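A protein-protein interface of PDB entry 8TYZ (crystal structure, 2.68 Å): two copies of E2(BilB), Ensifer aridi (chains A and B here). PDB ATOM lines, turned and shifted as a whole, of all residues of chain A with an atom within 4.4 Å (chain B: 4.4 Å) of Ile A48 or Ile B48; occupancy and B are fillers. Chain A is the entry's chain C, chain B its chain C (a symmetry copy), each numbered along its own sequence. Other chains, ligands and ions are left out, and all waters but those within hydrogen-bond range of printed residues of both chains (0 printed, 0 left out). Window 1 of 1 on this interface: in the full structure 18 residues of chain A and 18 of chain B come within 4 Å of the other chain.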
ATOM      1  N   GLY A  34      -0.518 -16.332  15.854  1.00  0.00           N
ATOM      2  CA  GLY A  34      -1.092 -17.568  15.378  1.00  0.00           C
ATOM      3  C   GLY A  34      -2.164 -17.422  14.323  1.00  0.00           C
ATOM      4  O   GLY A  34      -3.023 -18.308  14.219  1.00  0.00           O
ATOM      5  N   CYS A  35      -2.134 -16.353  13.528  1.00  0.00           N
ATOM      6  CA  CYS A  35      -3.181 -16.062  12.555  1.00  0.00           C
ATOM      7  C   CYS A  35      -2.602 -16.031  11.143  1.00  0.00           C
ATOM      8  O   CYS A  35      -1.787 -15.158  10.816  1.00  0.00           O
ATOM      9  CB  CYS A  35      -3.860 -14.734  12.885  1.00  0.00           C
ATOM     10  SG  CYS A  35      -5.182 -14.308  11.758  1.00  0.00           S
ATOM     11  N   PHE A  36      -3.050 -16.955  10.294  1.00  0.00           N
ATOM     12  CA  PHE A  36      -2.504 -17.088   8.949  1.00  0.00           C
ATOM     13  C   PHE A  36      -3.618 -16.941   7.931  1.00  0.00           C
ATOM     14  O   PHE A  36      -4.574 -17.718   7.944  1.00  0.00           O
ATOM     15  CB  PHE A  36      -1.809 -18.437   8.755  1.00  0.00           C
ATOM     16  CG  PHE A  36      -0.830 -18.799   9.846  1.00  0.00           C
ATOM     17  CD1 PHE A  36       0.517 -18.467   9.737  1.00  0.00           C
ATOM     18  CD2 PHE A  36      -1.251 -19.506  10.961  1.00  0.00           C
ATOM     19  CE1 PHE A  36       1.415 -18.816  10.730  1.00  0.00           C
ATOM     20  CE2 PHE A  36      -0.360 -19.857  11.954  1.00  0.00           C
ATOM     21  CZ  PHE A  36       0.973 -19.512  11.839  1.00  0.00           C
ATOM     22  N   ILE A  38      -4.904 -17.964   4.732  1.00  0.00           N
ATOM     23  CA  ILE A  38      -4.621 -19.065   3.825  1.00  0.00           C
ATOM     24  C   ILE A  38      -4.984 -18.700   2.394  1.00  0.00           C
ATOM     25  O   ILE A  38      -4.189 -18.918   1.470  1.00  0.00           O
ATOM     26  CB  ILE A  38      -5.348 -20.339   4.277  1.00  0.00           C
ATOM     27  CG1 ILE A  38      -4.845 -20.750   5.650  1.00  0.00           C
ATOM     28  CG2 ILE A  38      -5.082 -21.454   3.283  1.00  0.00           C
ATOM     29  CD1 ILE A  38      -3.352 -20.933   5.700  1.00  0.00           C
ATOM     30  N   PHE A  47      -8.903 -18.003   7.003  1.00  0.00           N
ATOM     31  CA  PHE A  47      -7.815 -17.941   7.959  1.00  0.00           C
ATOM     32  C   PHE A  47      -7.775 -19.241   8.739  1.00  0.00           C
ATOM     33  O   PHE A  47      -8.771 -19.964   8.831  1.00  0.00           O
ATOM     34  CB  PHE A  47      -7.984 -16.776   8.941  1.00  0.00           C
ATOM     35  CG  PHE A  47      -7.918 -15.431   8.304  1.00  0.00           C
ATOM     36  CD1 PHE A  47      -8.997 -14.932   7.583  1.00  0.00           C
ATOM     37  CD2 PHE A  47      -6.793 -14.653   8.445  1.00  0.00           C
ATOM     38  CE1 PHE A  47      -8.935 -13.692   6.997  1.00  0.00           C
ATOM     39  CE2 PHE A  47      -6.724 -13.422   7.866  1.00  0.00           C
ATOM     40  CZ  PHE A  47      -7.793 -12.935   7.141  1.00  0.00           C
ATOM     41  N   ILE A  48      -6.614 -19.532   9.307  1.00  0.00           N
ATOM     42  CA  ILE A  48      -6.495 -20.597  10.289  1.00  0.00           C
ATOM     43  C   ILE A  48      -5.848 -20.015  11.534  1.00  0.00           C
ATOM     44  O   ILE A  48      -5.092 -19.040  11.471  1.00  0.00           O
ATOM     45  CB  ILE A  48      -5.691 -21.808   9.769  1.00  0.00           C
ATOM     46  CG1 ILE A  48      -4.300 -21.379   9.310  1.00  0.00           C
ATOM     47  CG2 ILE A  48      -6.431 -22.523   8.640  1.00  0.00           C
ATOM     48  CD1 ILE A  48      -3.421 -22.542   8.978  1.00  0.00           C
ATOM     49  N   PHE A  49      -6.157 -20.623  12.675  1.00  0.00           N
ATOM     50  CA  PHE A  49      -5.720 -20.132  13.972  1.00  0.00           C
ATOM     51  C   PHE A  49      -5.067 -21.270  14.743  1.00  0.00           C
ATOM     52  O   PHE A  49      -5.643 -22.360  14.856  1.00  0.00           O
ATOM     53  CB  PHE A  49      -6.900 -19.536  14.771  1.00  0.00           C
ATOM     54  CG  PHE A  49      -7.512 -18.314  14.134  1.00  0.00           C
ATOM     55  CD1 PHE A  49      -6.974 -17.055  14.369  1.00  0.00           C
ATOM     56  CD2 PHE A  49      -8.603 -18.427  13.275  1.00  0.00           C
ATOM     57  CE1 PHE A  49      -7.515 -15.933  13.775  1.00  0.00           C
ATOM     58  CE2 PHE A  49      -9.146 -17.303  12.674  1.00  0.00           C
ATOM     59  CZ  PHE A  49      -8.600 -16.054  12.929  1.00  0.00           C
ATOM     60  N   ALA A  50      -3.856 -21.016  15.251  1.00  0.00           N
ATOM     61  CA  ALA A  50      -3.125 -21.941  16.111  1.00  0.00           C
ATOM     62  C   ALA A  50      -2.507 -21.147  17.251  1.00  0.00           C
ATOM     63  O   ALA A  50      -1.863 -20.124  17.008  1.00  0.00           O
ATOM     64  CB  ALA A  50      -2.030 -22.686  15.335  1.00  0.00           C
ATOM     65  N   ILE A  59      -3.956 -26.567  15.248  1.00  0.00           N
ATOM     66  CA  ILE A  59      -4.999 -25.788  14.597  1.00  0.00           C
ATOM     67  C   ILE A  59      -6.264 -25.880  15.442  1.00  0.00           C
ATOM     68  O   ILE A  59      -6.833 -26.967  15.608  1.00  0.00           O
ATOM     69  CB  ILE A  59      -5.227 -26.291  13.168  1.00  0.00           C
ATOM     70  CG1 ILE A  59      -3.910 -26.214  12.388  1.00  0.00           C
ATOM     71  CG2 ILE A  59      -6.353 -25.511  12.478  1.00  0.00           C
ATOM     72  CD1 ILE A  59      -4.079 -26.381  10.920  1.00  0.00           C
ATOM     73  N   ALA A  61      -8.891 -23.368  15.260  1.00  0.00           N
ATOM     74  CA  ALA A  61      -9.980 -22.623  14.646  1.00  0.00           C
ATOM     75  C   ALA A  61      -9.642 -22.376  13.183  1.00  0.00           C
ATOM     76  O   ALA A  61      -8.480 -22.138  12.842  1.00  0.00           O
ATOM     77  CB  ALA A  61     -10.216 -21.289  15.367  1.00  0.00           C
ATOM     78  N   ALA A  62     -10.657 -22.457  12.323  1.00  0.00           N
ATOM     79  CA  ALA A  62     -10.509 -22.114  10.916  1.00  0.00           C
ATOM     80  C   ALA A  62     -11.807 -21.473  10.477  1.00  0.00           C
ATOM     81  O   ALA A  62     -12.875 -22.052  10.681  1.00  0.00           O
ATOM     82  CB  ALA A  62     -10.196 -23.343  10.060  1.00  0.00           C
ATOM     83  N   PRO A  82     -10.602 -26.812   8.604  1.00  0.00           N
ATOM     84  CA  PRO A  82      -9.439 -26.216   7.917  1.00  0.00           C
ATOM     85  C   PRO A  82      -9.117 -26.848   6.570  1.00  0.00           C
ATOM     86  O   PRO A  82      -8.816 -26.121   5.619  1.00  0.00           O
ATOM     87  CB  PRO A  82      -8.296 -26.379   8.940  1.00  0.00           C
ATOM     88  CG  PRO A  82      -8.801 -27.293   9.995  1.00  0.00           C
ATOM     89  CD  PRO A  82     -10.293 -27.180   9.997  1.00  0.00           C
ATOM     90  N   GLY B  34      -3.183 -31.427   3.687  1.00  0.00           N
ATOM     91  CA  GLY B  34      -2.637 -30.713   4.816  1.00  0.00           C
ATOM     92  C   GLY B  34      -1.506 -29.763   4.499  1.00  0.00           C
ATOM     93  O   GLY B  34      -0.681 -29.501   5.385  1.00  0.00           O
ATOM     94  N   CYS B  35      -1.449 -29.226   3.281  1.00  0.00           N
ATOM     95  CA  CYS B  35      -0.340 -28.387   2.839  1.00  0.00           C
ATOM     96  C   CYS B  35      -0.842 -26.993   2.467  1.00  0.00           C
ATOM     97  O   CYS B  35      -1.601 -26.835   1.502  1.00  0.00           O
ATOM     98  CB  CYS B  35       0.375 -29.032   1.654  1.00  0.00           C
ATOM     99  SG  CYS B  35       1.772 -28.085   1.061  1.00  0.00           S
ATOM    100  N   PHE B  36      -0.389 -25.980   3.204  1.00  0.00           N
ATOM    101  CA  PHE B  36      -0.868 -24.618   3.009  1.00  0.00           C
ATOM    102  C   PHE B  36       0.303 -23.706   2.700  1.00  0.00           C
ATOM    103  O   PHE B  36       1.223 -23.586   3.510  1.00  0.00           O
ATOM    104  CB  PHE B  36      -1.609 -24.099   4.244  1.00  0.00           C
ATOM    105  CG  PHE B  36      -2.658 -25.040   4.785  1.00  0.00           C
ATOM    106  CD1 PHE B  36      -3.982 -24.950   4.366  1.00  0.00           C
ATOM    107  CD2 PHE B  36      -2.327 -25.986   5.741  1.00  0.00           C
ATOM    108  CE1 PHE B  36      -4.946 -25.802   4.876  1.00  0.00           C
ATOM    109  CE2 PHE B  36      -3.283 -26.838   6.254  1.00  0.00           C
ATOM    110  CZ  PHE B  36      -4.593 -26.746   5.822  1.00  0.00           C
ATOM    111  N   ILE B  38       1.712 -20.417   3.061  1.00  0.00           N
ATOM    112  CA  ILE B  38       1.431 -19.276   3.919  1.00  0.00           C
ATOM    113  C   ILE B  38       1.885 -17.979   3.267  1.00  0.00           C
ATOM    114  O   ILE B  38       1.131 -16.997   3.235  1.00  0.00           O
ATOM    115  CB  ILE B  38       2.078 -19.464   5.298  1.00  0.00           C
ATOM    116  CG1 ILE B  38       1.487 -20.688   5.974  1.00  0.00           C
ATOM    117  CG2 ILE B  38       1.819 -18.236   6.151  1.00  0.00           C
ATOM    118  CD1 ILE B  38      -0.013 -20.634   6.084  1.00  0.00           C
ATOM    119  N   PHE B  47       5.580 -22.788   3.810  1.00  0.00           N
ATOM    120  CA  PHE B  47       4.447 -23.688   3.902  1.00  0.00           C
ATOM    121  C   PHE B  47       4.311 -24.157   5.339  1.00  0.00           C
ATOM    122  O   PHE B  47       5.269 -24.127   6.116  1.00  0.00           O
ATOM    123  CB  PHE B  47       4.612 -24.910   2.993  1.00  0.00           C
ATOM    124  CG  PHE B  47       4.637 -24.586   1.539  1.00  0.00           C
ATOM    125  CD1 PHE B  47       5.773 -24.041   0.952  1.00  0.00           C
ATOM    126  CD2 PHE B  47       3.540 -24.849   0.753  1.00  0.00           C
ATOM    127  CE1 PHE B  47       5.795 -23.743  -0.389  1.00  0.00           C
ATOM    128  CE2 PHE B  47       3.554 -24.556  -0.578  1.00  0.00           C
ATOM    129  CZ  PHE B  47       4.679 -24.003  -1.155  1.00  0.00           C
ATOM    130  N   ILE B  48       3.110 -24.596   5.686  1.00  0.00           N
ATOM    131  CA  ILE B  48       2.894 -25.311   6.933  1.00  0.00           C
ATOM    132  C   ILE B  48       2.208 -26.626   6.606  1.00  0.00           C
ATOM    133  O   ILE B  48       1.497 -26.750   5.602  1.00  0.00           O
ATOM    134  CB  ILE B  48       2.068 -24.501   7.956  1.00  0.00           C
ATOM    135  CG1 ILE B  48       0.723 -24.090   7.363  1.00  0.00           C
ATOM    136  CG2 ILE B  48       2.836 -23.273   8.443  1.00  0.00           C
ATOM    137  CD1 ILE B  48      -0.185 -23.472   8.376  1.00  0.00           C
ATOM    138  N   PHE B  49       2.430 -27.615   7.465  1.00  0.00           N
ATOM    139  CA  PHE B  49       1.946 -28.969   7.249  1.00  0.00           C
ATOM    140  C   PHE B  49       1.206 -29.439   8.493  1.00  0.00           C
ATOM    141  O   PHE B  49       1.728 -29.332   9.610  1.00  0.00           O
ATOM    142  CB  PHE B  49       3.106 -29.930   6.908  1.00  0.00           C
ATOM    143  CG  PHE B  49       3.802 -29.607   5.609  1.00  0.00           C
ATOM    144  CD1 PHE B  49       3.306 -30.093   4.406  1.00  0.00           C
ATOM    145  CD2 PHE B  49       4.931 -28.791   5.587  1.00  0.00           C
ATOM    146  CE1 PHE B  49       3.924 -29.787   3.211  1.00  0.00           C
ATOM    147  CE2 PHE B  49       5.552 -28.478   4.389  1.00  0.00           C
ATOM    148  CZ  PHE B  49       5.046 -28.982   3.200  1.00  0.00           C
ATOM    149  N   ALA B  50      -0.019 -29.940   8.293  1.00  0.00           N
ATOM    150  CA  ALA B  50      -0.832 -30.540   9.345  1.00  0.00           C
ATOM    151  C   ALA B  50      -1.476 -31.801   8.790  1.00  0.00           C
ATOM    152  O   ALA B  50      -2.063 -31.765   7.706  1.00  0.00           O
ATOM    153  CB  ALA B  50      -1.916 -29.572   9.842  1.00  0.00           C
ATOM    154  N   ILE B  59      -0.153 -28.706  13.705  1.00  0.00           N
ATOM    155  CA  ILE B  59       0.955 -28.290  12.859  1.00  0.00           C
ATOM    156  C   ILE B  59       2.168 -29.145  13.200  1.00  0.00           C
ATOM    157  O   ILE B  59       2.681 -29.089  14.326  1.00  0.00           O
ATOM    158  CB  ILE B  59       1.237 -26.795  13.045  1.00  0.00           C
ATOM    159  CG1 ILE B  59      -0.033 -25.997  12.729  1.00  0.00           C
ATOM    160  CG2 ILE B  59       2.429 -26.344  12.194  1.00  0.00           C
ATOM    161  CD1 ILE B  59       0.206 -24.537  12.578  1.00  0.00           C
ATOM    162  N   ALA B  61       4.904 -29.637  10.853  1.00  0.00           N
ATOM    163  CA  ALA B  61       6.055 -29.251  10.050  1.00  0.00           C
ATOM    164  C   ALA B  61       5.806 -27.867   9.469  1.00  0.00           C
ATOM    165  O   ALA B  61       4.674 -27.539   9.101  1.00  0.00           O
ATOM    166  CB  ALA B  61       6.309 -30.261   8.922  1.00  0.00           C
ATOM    167  N   ALA B  62       6.860 -27.054   9.412  1.00  0.00           N
ATOM    168  CA  ALA B  62       6.802 -25.754   8.761  1.00  0.00           C
ATOM    169  C   ALA B  62       8.147 -25.523   8.108  1.00  0.00           C
ATOM    170  O   ALA B  62       9.178 -25.639   8.774  1.00  0.00           O
ATOM    171  CB  ALA B  62       6.483 -24.634   9.753  1.00  0.00           C
ATOM    172  N   PRO B  82       6.819 -22.461  12.833  1.00  0.00           N
ATOM    173  CA  PRO B  82       5.720 -21.876  12.039  1.00  0.00           C
ATOM    174  C   PRO B  82       5.443 -20.409  12.342  1.00  0.00           C
ATOM    175  O   PRO B  82       5.223 -19.632  11.408  1.00  0.00           O
ATOM    176  CB  PRO B  82       4.519 -22.787  12.363  1.00  0.00           C
ATOM    177  CG  PRO B  82       4.927 -23.632  13.512  1.00  0.00           C
ATOM    178  CD  PRO B  82       6.421 -23.723  13.481  1.00  0.00           C
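O of Phe A36 is in hydrogen-bond range of N of Ile A48. The backbone NH (N) of Ile B48 is in hydrogen-bond range of the backbone carbonyl oxygen (O) of Phe B36, at 3.1 Å.
Gly A34 touches none of the printed residues of chain B. Of the printed residues of chain B, Phe A36 touches Ile B38 and Pro B82. Of the printed residues of chain B, Ile A48 touches Ile B48. Of the printed residues of chain A, Ile B38 touches Phe A36 and Ile A38. Of the printed residues of chain A, Ile B59 touches Ile A59 (3.9 Å). The nearest printed residue of chain A that does not touch Ile B48 is Phe A36 (4.9 Å).
Of the 12 printed residues of chain A, 5 touch a printed residue of chain B. Hydrophobic or aromatic side chains of chain A within 4 Å of the printed part of chain B: Phe A36, Ile A38, Ile A48 and Ile A59. Along chain A the printed residues that touch a printed residue of chain B span positions 36 to 82. Of the 12 printed residues of chain B, 5 touch a printed residue of chain A. Printed residues of chain B that touch a printed residue of chain A: Phe B36, Ile B38, Ile B48, Ile B59 and Pro B82. Hydrophobic or aromatic side chains of chain B that line the printed part of chain A: Phe B36, Ile B38, Ile B48 and Ile B59. Among the printed residues, 7 pairs touch across the chains.
Among the printed residues, merely in contact across the chains: Ile A38 with Ile B38, Ile A48 with Ile B48, Ile A38 with Phe B36, Phe A36 with Ile B38, Ile A59 with Ile B59, Phe A36 with Pro B82 and Pro A82 with Phe B36.
Phe A36 touches Ile B38, and with the chains exchanged Ile A38 touches Phe B36. Phe A36 touches Pro B82, and with the chains exchanged Pro A82 touches Phe B36. Ile B38 touches its own counterpart, Ile A38. Ile B48 touches its own counterpart, Ile A48.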
